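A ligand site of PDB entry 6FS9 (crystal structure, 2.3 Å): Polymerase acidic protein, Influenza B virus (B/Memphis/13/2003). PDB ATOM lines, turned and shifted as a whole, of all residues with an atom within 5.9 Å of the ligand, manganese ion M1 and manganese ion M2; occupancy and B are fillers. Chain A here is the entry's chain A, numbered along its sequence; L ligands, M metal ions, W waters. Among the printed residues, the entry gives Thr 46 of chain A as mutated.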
ATOM      1  N   ALA A  25     -28.905 -25.406   1.624  1.00  0.00           N
ATOM      2  CA  ALA A  25     -29.127 -25.559   0.198  1.00  0.00           C
ATOM      3  C   ALA A  25     -29.562 -24.194  -0.424  1.00  0.00           C
ATOM      4  O   ALA A  25     -29.152 -23.853  -1.520  1.00  0.00           O
ATOM      5  CB  ALA A  25     -30.110 -26.650  -0.059  1.00  0.00           C
ATOM      6  N   THR A  28     -26.655 -21.958  -0.757  1.00  0.00           N
ATOM      7  CA  THR A  28     -25.938 -22.302  -1.956  1.00  0.00           C
ATOM      8  C   THR A  28     -26.643 -21.790  -3.227  1.00  0.00           C
ATOM      9  O   THR A  28     -25.999 -21.277  -4.139  1.00  0.00           O
ATOM     10  CB  THR A  28     -25.794 -23.810  -2.058  1.00  0.00           C
ATOM     11  OG1 THR A  28     -25.052 -24.249  -0.928  1.00  0.00           O
ATOM     12  CG2 THR A  28     -24.997 -24.177  -3.277  1.00  0.00           C
ATOM     13  N   MET A  29     -27.956 -21.941  -3.311  1.00  0.00           N
ATOM     14  CA  MET A  29     -28.659 -21.477  -4.510  1.00  0.00           C
ATOM     15  C   MET A  29     -28.460 -19.950  -4.675  1.00  0.00           C
ATOM     16  O   MET A  29     -28.292 -19.460  -5.773  1.00  0.00           O
ATOM     17  CB  MET A  29     -30.155 -21.852  -4.475  1.00  0.00           C
ATOM     18  CG  MET A  29     -30.454 -23.310  -4.780  1.00  0.00           C
ATOM     19  SD  MET A  29     -32.168 -23.778  -4.398  1.00  0.00           S
ATOM     20  CE  MET A  29     -33.094 -23.023  -5.746  1.00  0.00           C
ATOM     21  N   ALA A  30     -28.513 -19.218  -3.574  1.00  0.00           N
ATOM     22  CA  ALA A  30     -28.258 -17.763  -3.537  1.00  0.00           C
ATOM     23  C   ALA A  30     -26.870 -17.365  -4.099  1.00  0.00           C
ATOM     24  O   ALA A  30     -26.733 -16.399  -4.828  1.00  0.00           O
ATOM     25  CB  ALA A  30     -28.442 -17.220  -2.099  1.00  0.00           C
ATOM     26  N   PHE A  32     -25.240 -18.794  -6.338  1.00  0.00           N
ATOM     27  CA  PHE A  32     -25.484 -18.882  -7.798  1.00  0.00           C
ATOM     28  C   PHE A  32     -26.609 -17.962  -8.338  1.00  0.00           C
ATOM     29  O   PHE A  32     -27.076 -18.131  -9.451  1.00  0.00           O
ATOM     30  CB  PHE A  32     -25.737 -20.379  -8.157  1.00  0.00           C
ATOM     31  CG  PHE A  32     -24.503 -21.237  -8.056  1.00  0.00           C
ATOM     32  CD1 PHE A  32     -23.491 -21.115  -9.000  1.00  0.00           C
ATOM     33  CD2 PHE A  32     -24.308 -22.105  -6.991  1.00  0.00           C
ATOM     34  CE1 PHE A  32     -22.328 -21.881  -8.912  1.00  0.00           C
ATOM     35  CE2 PHE A  32     -23.151 -22.872  -6.886  1.00  0.00           C
ATOM     36  CZ  PHE A  32     -22.151 -22.755  -7.842  1.00  0.00           C
ATOM     37  N   GLU A  34     -29.739 -18.255  -7.744  1.00  0.00           N
ATOM     38  CA  GLU A  34     -30.992 -18.943  -8.041  1.00  0.00           C
ATOM     39  C   GLU A  34     -31.866 -18.729  -6.829  1.00  0.00           C
ATOM     40  O   GLU A  34     -31.396 -18.733  -5.699  1.00  0.00           O
ATOM     41  CB  GLU A  34     -30.789 -20.419  -8.340  1.00  0.00           C
ATOM     42  CG  GLU A  34     -30.016 -20.700  -9.617  1.00  0.00           C
ATOM     43  CD  GLU A  34     -30.755 -20.338 -10.890  1.00  0.00           C
ATOM     44  OE1 GLU A  34     -31.989 -20.519 -10.970  1.00  0.00           O
ATOM     45  OE2 GLU A  34     -30.048 -19.877 -11.807  1.00  0.00           O
ATOM     46  N   MET A  42     -35.075 -27.314  -7.811  1.00  0.00           N
ATOM     47  CA  MET A  42     -33.664 -27.225  -7.513  1.00  0.00           C
ATOM     48  C   MET A  42     -33.465 -27.289  -6.023  1.00  0.00           C
ATOM     49  O   MET A  42     -32.530 -27.958  -5.517  1.00  0.00           O
ATOM     50  CB  MET A  42     -33.091 -25.935  -8.075  1.00  0.00           C
ATOM     51  CG  MET A  42     -31.579 -25.778  -7.930  1.00  0.00           C
ATOM     52  SD  MET A  42     -30.986 -24.298  -8.741  1.00  0.00           S
ATOM     53  CE  MET A  42     -31.183 -24.855 -10.451  1.00  0.00           C
ATOM     54  N   ASN A  45     -33.729 -30.921  -4.961  1.00  0.00           N
ATOM     55  CA  ASN A  45     -32.612 -31.732  -5.432  1.00  0.00           C
ATOM     56  C   ASN A  45     -31.341 -31.469  -4.650  1.00  0.00           C
ATOM     57  O   ASN A  45     -30.596 -32.431  -4.379  1.00  0.00           O
ATOM     58  CB  ASN A  45     -32.345 -31.484  -6.894  1.00  0.00           C
ATOM     59  CG  ASN A  45     -33.430 -32.045  -7.773  1.00  0.00           C
ATOM     60  OD1 ASN A  45     -34.030 -33.080  -7.466  1.00  0.00           O
ATOM     61  ND2 ASN A  45     -33.676 -31.390  -8.878  1.00  0.00           N
ATOM     62  N   THR A  46     -31.172 -30.206  -4.234  1.00  0.00           N
ATOM     63  CA  THR A  46     -29.983 -29.797  -3.515  1.00  0.00           C
ATOM     64  C   THR A  46     -30.134 -30.260  -2.089  1.00  0.00           C
ATOM     65  O   THR A  46     -29.141 -30.617  -1.457  1.00  0.00           O
ATOM     66  CB  THR A  46     -29.682 -28.278  -3.590  1.00  0.00           C
ATOM     67  OG1 THR A  46     -30.822 -27.537  -3.229  1.00  0.00           O
ATOM     68  CG2 THR A  46     -29.315 -27.851  -4.996  1.00  0.00           C
ATOM     69  N   HIS A  49     -29.304 -34.045  -2.146  1.00  0.00           N
ATOM     70  CA  HIS A  49     -27.861 -34.273  -2.370  1.00  0.00           C
ATOM     71  C   HIS A  49     -27.090 -33.991  -1.099  1.00  0.00           C
ATOM     72  O   HIS A  49     -26.306 -34.821  -0.651  1.00  0.00           O
ATOM     73  CB  HIS A  49     -27.395 -33.377  -3.468  1.00  0.00           C
ATOM     74  CG  HIS A  49     -25.930 -33.441  -3.755  1.00  0.00           C
ATOM     75  ND1 HIS A  49     -25.064 -32.489  -3.295  1.00  0.00           N
ATOM     76  CD2 HIS A  49     -25.212 -34.245  -4.541  1.00  0.00           C
ATOM     77  CE1 HIS A  49     -23.863 -32.741  -3.737  1.00  0.00           C
ATOM     78  NE2 HIS A  49     -23.915 -33.812  -4.494  1.00  0.00           N
ATOM     79  N   CYS A  53     -25.058 -36.638   1.408  1.00  0.00           N
ATOM     80  CA  CYS A  53     -23.704 -36.371   1.875  1.00  0.00           C
ATOM     81  C   CYS A  53     -23.614 -36.523   3.369  1.00  0.00           C
ATOM     82  O   CYS A  53     -22.738 -37.245   3.865  1.00  0.00           O
ATOM     83  CB  CYS A  53     -23.228 -34.962   1.497  1.00  0.00           C
ATOM     84  SG  CYS A  53     -22.935 -34.693  -0.265  1.00  0.00           S
ATOM     85  N   GLU A  89     -19.436 -30.115   0.711  1.00  0.00           N
ATOM     86  CA  GLU A  89     -20.702 -29.591   0.204  1.00  0.00           C
ATOM     87  C   GLU A  89     -21.441 -28.849   1.337  1.00  0.00           C
ATOM     88  O   GLU A  89     -21.253 -29.159   2.507  1.00  0.00           O
ATOM     89  CB  GLU A  89     -21.583 -30.736  -0.343  1.00  0.00           C
ATOM     90  CG  GLU A  89     -22.871 -30.273  -1.077  1.00  0.00           C
ATOM     91  CD  GLU A  89     -22.607 -29.204  -2.152  1.00  0.00           C
ATOM     92  OE1 GLU A  89     -22.541 -29.596  -3.354  1.00  0.00           O
ATOM     93  OE2 GLU A  89     -22.459 -27.984  -1.798  1.00  0.00           O
ATOM     94  N   ARG A  93     -18.639 -21.376  -1.242  1.00  0.00           N
ATOM     95  CA  ARG A  93     -17.525 -21.830  -2.068  1.00  0.00           C
ATOM     96  C   ARG A  93     -16.151 -21.322  -1.647  1.00  0.00           C
ATOM     97  O   ARG A  93     -15.162 -22.049  -1.806  1.00  0.00           O
ATOM     98  CB  ARG A  93     -17.782 -21.545  -3.549  1.00  0.00           C
ATOM     99  CG  ARG A  93     -18.846 -22.470  -4.060  1.00  0.00           C
ATOM    100  CD  ARG A  93     -19.004 -22.336  -5.547  1.00  0.00           C
ATOM    101  NE  ARG A  93     -17.971 -23.045  -6.292  1.00  0.00           N
ATOM    102  CZ  ARG A  93     -18.061 -24.311  -6.657  1.00  0.00           C
ATOM    103  NH1 ARG A  93     -19.092 -25.049  -6.314  1.00  0.00           N
ATOM    104  NH2 ARG A  93     -17.120 -24.880  -7.382  1.00  0.00           N
ATOM    105  N   LEU A 115     -14.491 -28.667  -7.132  1.00  0.00           N
ATOM    106  CA  LEU A 115     -14.877 -28.744  -5.721  1.00  0.00           C
ATOM    107  C   LEU A 115     -15.634 -30.033  -5.457  1.00  0.00           C
ATOM    108  O   LEU A 115     -16.543 -30.349  -6.186  1.00  0.00           O
ATOM    109  CB  LEU A 115     -15.749 -27.548  -5.359  1.00  0.00           C
ATOM    110  CG  LEU A 115     -15.992 -27.239  -3.892  1.00  0.00           C
ATOM    111  CD1 LEU A 115     -14.695 -26.749  -3.278  1.00  0.00           C
ATOM    112  CD2 LEU A 115     -17.074 -26.176  -3.740  1.00  0.00           C
ATOM    113  N   ALA A 116     -15.213 -30.779  -4.446  1.00  0.00           N
ATOM    114  CA  ALA A 116     -15.765 -32.081  -4.082  1.00  0.00           C
ATOM    115  C   ALA A 116     -16.916 -31.936  -3.119  1.00  0.00           C
ATOM    116  O   ALA A 116     -17.164 -30.873  -2.564  1.00  0.00           O
ATOM    117  CB  ALA A 116     -14.686 -32.919  -3.429  1.00  0.00           C
ATOM    118  N   ASP A 117     -17.557 -33.053  -2.880  1.00  0.00           N
ATOM    119  CA  ASP A 117     -18.664 -33.142  -1.914  1.00  0.00           C
ATOM    120  C   ASP A 117     -18.157 -33.613  -0.588  1.00  0.00           C
ATOM    121  O   ASP A 117     -18.601 -33.068   0.427  1.00  0.00           O
ATOM    122  CB  ASP A 117     -19.760 -34.050  -2.437  1.00  0.00           C
ATOM    123  CG  ASP A 117     -20.501 -33.434  -3.649  1.00  0.00           C
ATOM    124  OD1 ASP A 117     -20.622 -32.209  -3.615  1.00  0.00           O
ATOM    125  OD2 ASP A 117     -20.962 -34.138  -4.617  1.00  0.00           O
ATOM    126  N   GLU A 128     -16.972 -37.207  -4.997  1.00  0.00           N
ATOM    127  CA  GLU A 128     -18.088 -36.557  -5.639  1.00  0.00           C
ATOM    128  C   GLU A 128     -19.290 -37.513  -5.428  1.00  0.00           C
ATOM    129  O   GLU A 128     -19.250 -38.683  -5.789  1.00  0.00           O
ATOM    130  CB  GLU A 128     -17.837 -36.378  -7.132  1.00  0.00           C
ATOM    131  CG  GLU A 128     -19.079 -35.878  -7.932  1.00  0.00           C
ATOM    132  CD  GLU A 128     -19.589 -34.502  -7.434  1.00  0.00           C
ATOM    133  OE1 GLU A 128     -18.735 -33.701  -6.987  1.00  0.00           O
ATOM    134  OE2 GLU A 128     -20.806 -34.225  -7.458  1.00  0.00           O
ATOM    135  N   VAL A 129     -20.365 -36.953  -4.858  1.00  0.00           N
ATOM    136  CA  VAL A 129     -21.646 -37.586  -4.698  1.00  0.00           C
ATOM    137  C   VAL A 129     -22.580 -37.106  -5.789  1.00  0.00           C
ATOM    138  O   VAL A 129     -22.646 -35.905  -6.103  1.00  0.00           O
ATOM    139  CB  VAL A 129     -22.255 -37.274  -3.334  1.00  0.00           C
ATOM    140  CG1 VAL A 129     -23.588 -37.942  -3.174  1.00  0.00           C
ATOM    141  CG2 VAL A 129     -21.293 -37.648  -2.191  1.00  0.00           C
ATOM    142  N   GLY A 130     -23.270 -38.067  -6.391  1.00  0.00           N
ATOM    143  CA  GLY A 130     -24.230 -37.823  -7.458  1.00  0.00           C
ATOM    144  C   GLY A 130     -25.574 -38.496  -7.171  1.00  0.00           C
ATOM    145  O   GLY A 130     -25.627 -39.641  -6.681  1.00  0.00           O
ATOM    146  N   ILE A 131     -26.658 -37.789  -7.471  1.00  0.00           N
ATOM    147  CA  ILE A 131     -28.009 -38.359  -7.321  1.00  0.00           C
ATOM    148  C   ILE A 131     -28.679 -38.278  -8.655  1.00  0.00           C
ATOM    149  O   ILE A 131     -28.663 -37.261  -9.266  1.00  0.00           O
ATOM    150  CB  ILE A 131     -28.861 -37.600  -6.306  1.00  0.00           C
ATOM    151  CG1 ILE A 131     -28.147 -37.413  -4.967  1.00  0.00           C
ATOM    152  CG2 ILE A 131     -30.175 -38.339  -6.045  1.00  0.00           C
ATOM    153  CD1 ILE A 131     -27.890 -38.671  -4.194  1.00  0.00           C
ATOM    154  N   TYR A 139     -24.879 -41.838 -15.186  1.00  0.00           N
ATOM    155  CA  TYR A 139     -24.471 -40.644 -14.444  1.00  0.00           C
ATOM    156  C   TYR A 139     -23.012 -40.788 -13.911  1.00  0.00           C
ATOM    157  O   TYR A 139     -22.257 -39.839 -13.902  1.00  0.00           O
ATOM    158  CB  TYR A 139     -25.508 -40.333 -13.344  1.00  0.00           C
ATOM    159  CG  TYR A 139     -25.453 -38.936 -12.750  1.00  0.00           C
ATOM    160  CD1 TYR A 139     -25.359 -37.787 -13.548  1.00  0.00           C
ATOM    161  CD2 TYR A 139     -25.500 -38.755 -11.391  1.00  0.00           C
ATOM    162  CE1 TYR A 139     -25.286 -36.514 -12.976  1.00  0.00           C
ATOM    163  CE2 TYR A 139     -25.462 -37.503 -10.817  1.00  0.00           C
ATOM    164  CZ  TYR A 139     -25.336 -36.393 -11.593  1.00  0.00           C
ATOM    165  OH  TYR A 139     -25.278 -35.182 -10.952  1.00  0.00           O
ATOM    166  N   LYS A 143     -20.054 -38.019 -15.043  1.00  0.00           N
ATOM    167  CA  LYS A 143     -19.266 -37.373 -13.993  1.00  0.00           C
ATOM    168  C   LYS A 143     -17.769 -37.590 -14.251  1.00  0.00           C
ATOM    169  O   LYS A 143     -16.971 -36.684 -14.092  1.00  0.00           O
ATOM    170  CB  LYS A 143     -19.621 -37.920 -12.632  1.00  0.00           C
ATOM    171  CG  LYS A 143     -20.939 -37.425 -12.077  1.00  0.00           C
ATOM    172  CD  LYS A 143     -20.766 -36.158 -11.248  1.00  0.00           C
ATOM    173  CE  LYS A 143     -22.092 -35.680 -10.660  1.00  0.00           C
ATOM    174  NZ  LYS A 143     -21.976 -34.470  -9.790  1.00  0.00           N
HETATM  175  C1  LIG L   1     -23.792 -32.424  -8.073  1.00  0.00           C
HETATM  176  N1  LIG L   1     -24.306 -29.779  -8.763  1.00  0.00           N
HETATM  177  O1  LIG L   1     -23.533 -33.586  -7.722  1.00  0.00           O
HETATM  178  C2  LIG L   1     -24.792 -32.101  -8.961  1.00  0.00           C
HETATM  179  O2  LIG L   1     -22.147 -31.687  -6.660  1.00  0.00           O
HETATM  180  O3  LIG L   1     -21.619 -28.936  -6.443  1.00  0.00           O
HETATM  181  C3  LIG L   1     -23.296 -30.025  -7.808  1.00  0.00           C
HETATM  182  O4  LIG L   1     -21.785 -26.578 -10.341  1.00  0.00           O
HETATM  183  C4  LIG L   1     -23.014 -31.345  -7.468  1.00  0.00           C
HETATM  184  C5  LIG L   1     -22.510 -28.834  -7.271  1.00  0.00           C
HETATM  185  C6  LIG L   1     -23.640 -27.459  -8.993  1.00  0.00           C
HETATM  186  C7  LIG L   1     -26.855 -26.142  -9.008  1.00  0.00           C
HETATM  187  C8  LIG L   1     -27.019 -26.985 -10.269  1.00  0.00           C
HETATM  188  C9  LIG L   1     -27.851 -29.198  -8.523  1.00  0.00           C
HETATM  189  C10 LIG L   1     -26.732 -29.060  -7.701  1.00  0.00           C
HETATM  190  C11 LIG L   1     -28.717 -30.265  -8.276  1.00  0.00           C
HETATM  191  C12 LIG L   1     -28.496 -31.154  -7.227  1.00  0.00           C
HETATM  192  C13 LIG L   1     -27.406 -30.997  -6.403  1.00  0.00           C
HETATM  193  C14 LIG L   1     -26.529 -29.957  -6.648  1.00  0.00           C
HETATM  194  C15 LIG L   1     -26.258 -25.893  -6.680  1.00  0.00           C
HETATM  195  C16 LIG L   1     -26.778 -24.574  -6.660  1.00  0.00           C
HETATM  196  C17 LIG L   1     -27.337 -24.067  -7.835  1.00  0.00           C
HETATM  197  C18 LIG L   1     -27.368 -24.835  -8.973  1.00  0.00           C
HETATM  198  F1  LIG L   1     -27.847 -22.858  -7.933  1.00  0.00           F
HETATM  199  C19 LIG L   1     -26.287 -26.685  -7.852  1.00  0.00           C
HETATM  200  F2  LIG L   1     -27.926 -24.260 -10.042  1.00  0.00           F
HETATM  201  S1  LIG L   1     -28.280 -28.233  -9.853  1.00  0.00           S
HETATM  202  C20 LIG L   1     -25.686 -28.054  -7.844  1.00  0.00           C
HETATM  203  N2  LIG L   1     -24.720 -28.442  -8.992  1.00  0.00           N
HETATM  204  C21 LIG L   1     -22.889 -27.525 -10.340  1.00  0.00           C
HETATM  205  C22 LIG L   1     -20.940 -26.682  -9.133  1.00  0.00           C
HETATM  206  C23 LIG L   1     -21.764 -26.533  -7.820  1.00  0.00           C
HETATM  207  N3  LIG L   1     -22.667 -27.665  -7.905  1.00  0.00           N
HETATM  208  C24 LIG L   1     -25.014 -30.757  -9.287  1.00  0.00           C
HETATM  209 MN    MN M   1     -22.342 -33.857  -5.991  1.00  0.00          MN
HETATM  210 MN    MN M   2     -20.904 -30.536  -4.877  1.00  0.00          MN
HETATM  211  O   HOH W   1     -19.304 -31.344  -6.484  1.00  0.00           O
HETATM  212  O   HOH W   2     -25.987 -35.083  -8.243  1.00  0.00           O
HETATM  213  O   HOH W   3     -19.342 -29.356  -3.750  1.00  0.00           O
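The side-chain amino group of Lys 143 lies close to an oxygen (O1) of the ligand, at 2.7 Å.
The side-chain carboxylate (OE2) of Glu 128 sits close to the side-chain amino group (NZ) of Lys 143, at 2.6 Å. SG of Cys 53 lies within hydrogen-bond range of O of His 49 (3.4 Å). O of Met 42 sits at hydrogen-bond distance from OG1 of Thr 46 (2.9 Å). The backbone NH of Glu 34 is in hydrogen-bond range of the backbone carbonyl oxygen of Met 29 (2.7 Å).
SD of Met 42 lies close to F2 of the ligand (3.3 Å). Residues that only touch the ligand: Thr 28, Met 29, Phe 32, Glu 34, Asn 45, Thr 46, Arg 93 and Tyr 139. Of the 22 residues printed, 15 come within 4 Å of the ligand.
Residues that only touch manganese ion M1: Lys 143. Within 4 Å of manganese ion M1: His 49, Asp 117, Glu 128, Val 129 and Lys 143.
Within 4 Å of manganese ion M2: His 49, Glu 89 and Asp 117. Along chain A the residues within 4 Å of manganese ion M2 span positions 49 to 117. The nearest printed residue that does not touch manganese ion M2 is Glu 128 (4.4 Å).
The side-chain carboxylate (OD2) of Asp 117 is bound to manganese ion M1 (2.0 Å). The backbone carbonyl oxygen (O) of Val 129 binds manganese ion M1 (2.1 Å). Manganese ion M1 is bound by O1 of the ligand, at 2.1 Å. OE2 of Glu 128 is bound to manganese ion M1 (2.2 Å). A ring nitrogen (NE2) of His 49 is bound to manganese ion M1, at 2.2 Å. O2 of the ligand binds manganese ion M1 (2.3 Å).
Manganese ion M2 is bound by OD1 of Asp 117 (2.1 Å), water W3 (2.3 Å), O3 of the ligand (2.4 Å), water W1 (2.4 Å), OE1 of Glu 89 (2.4 Å) and O2 of the ligand (2.5 Å).
Water W1 lies within hydrogen-bond range of OE1 of Glu 128 (2.5 Å) and O of Leu 115 (2.9 Å). Water W2 lies within hydrogen-bond range of the side-chain hydroxyl (OH) of Tyr 139 (2.8 Å) and the backbone NH (N) of Ile 131 (2.9 Å).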
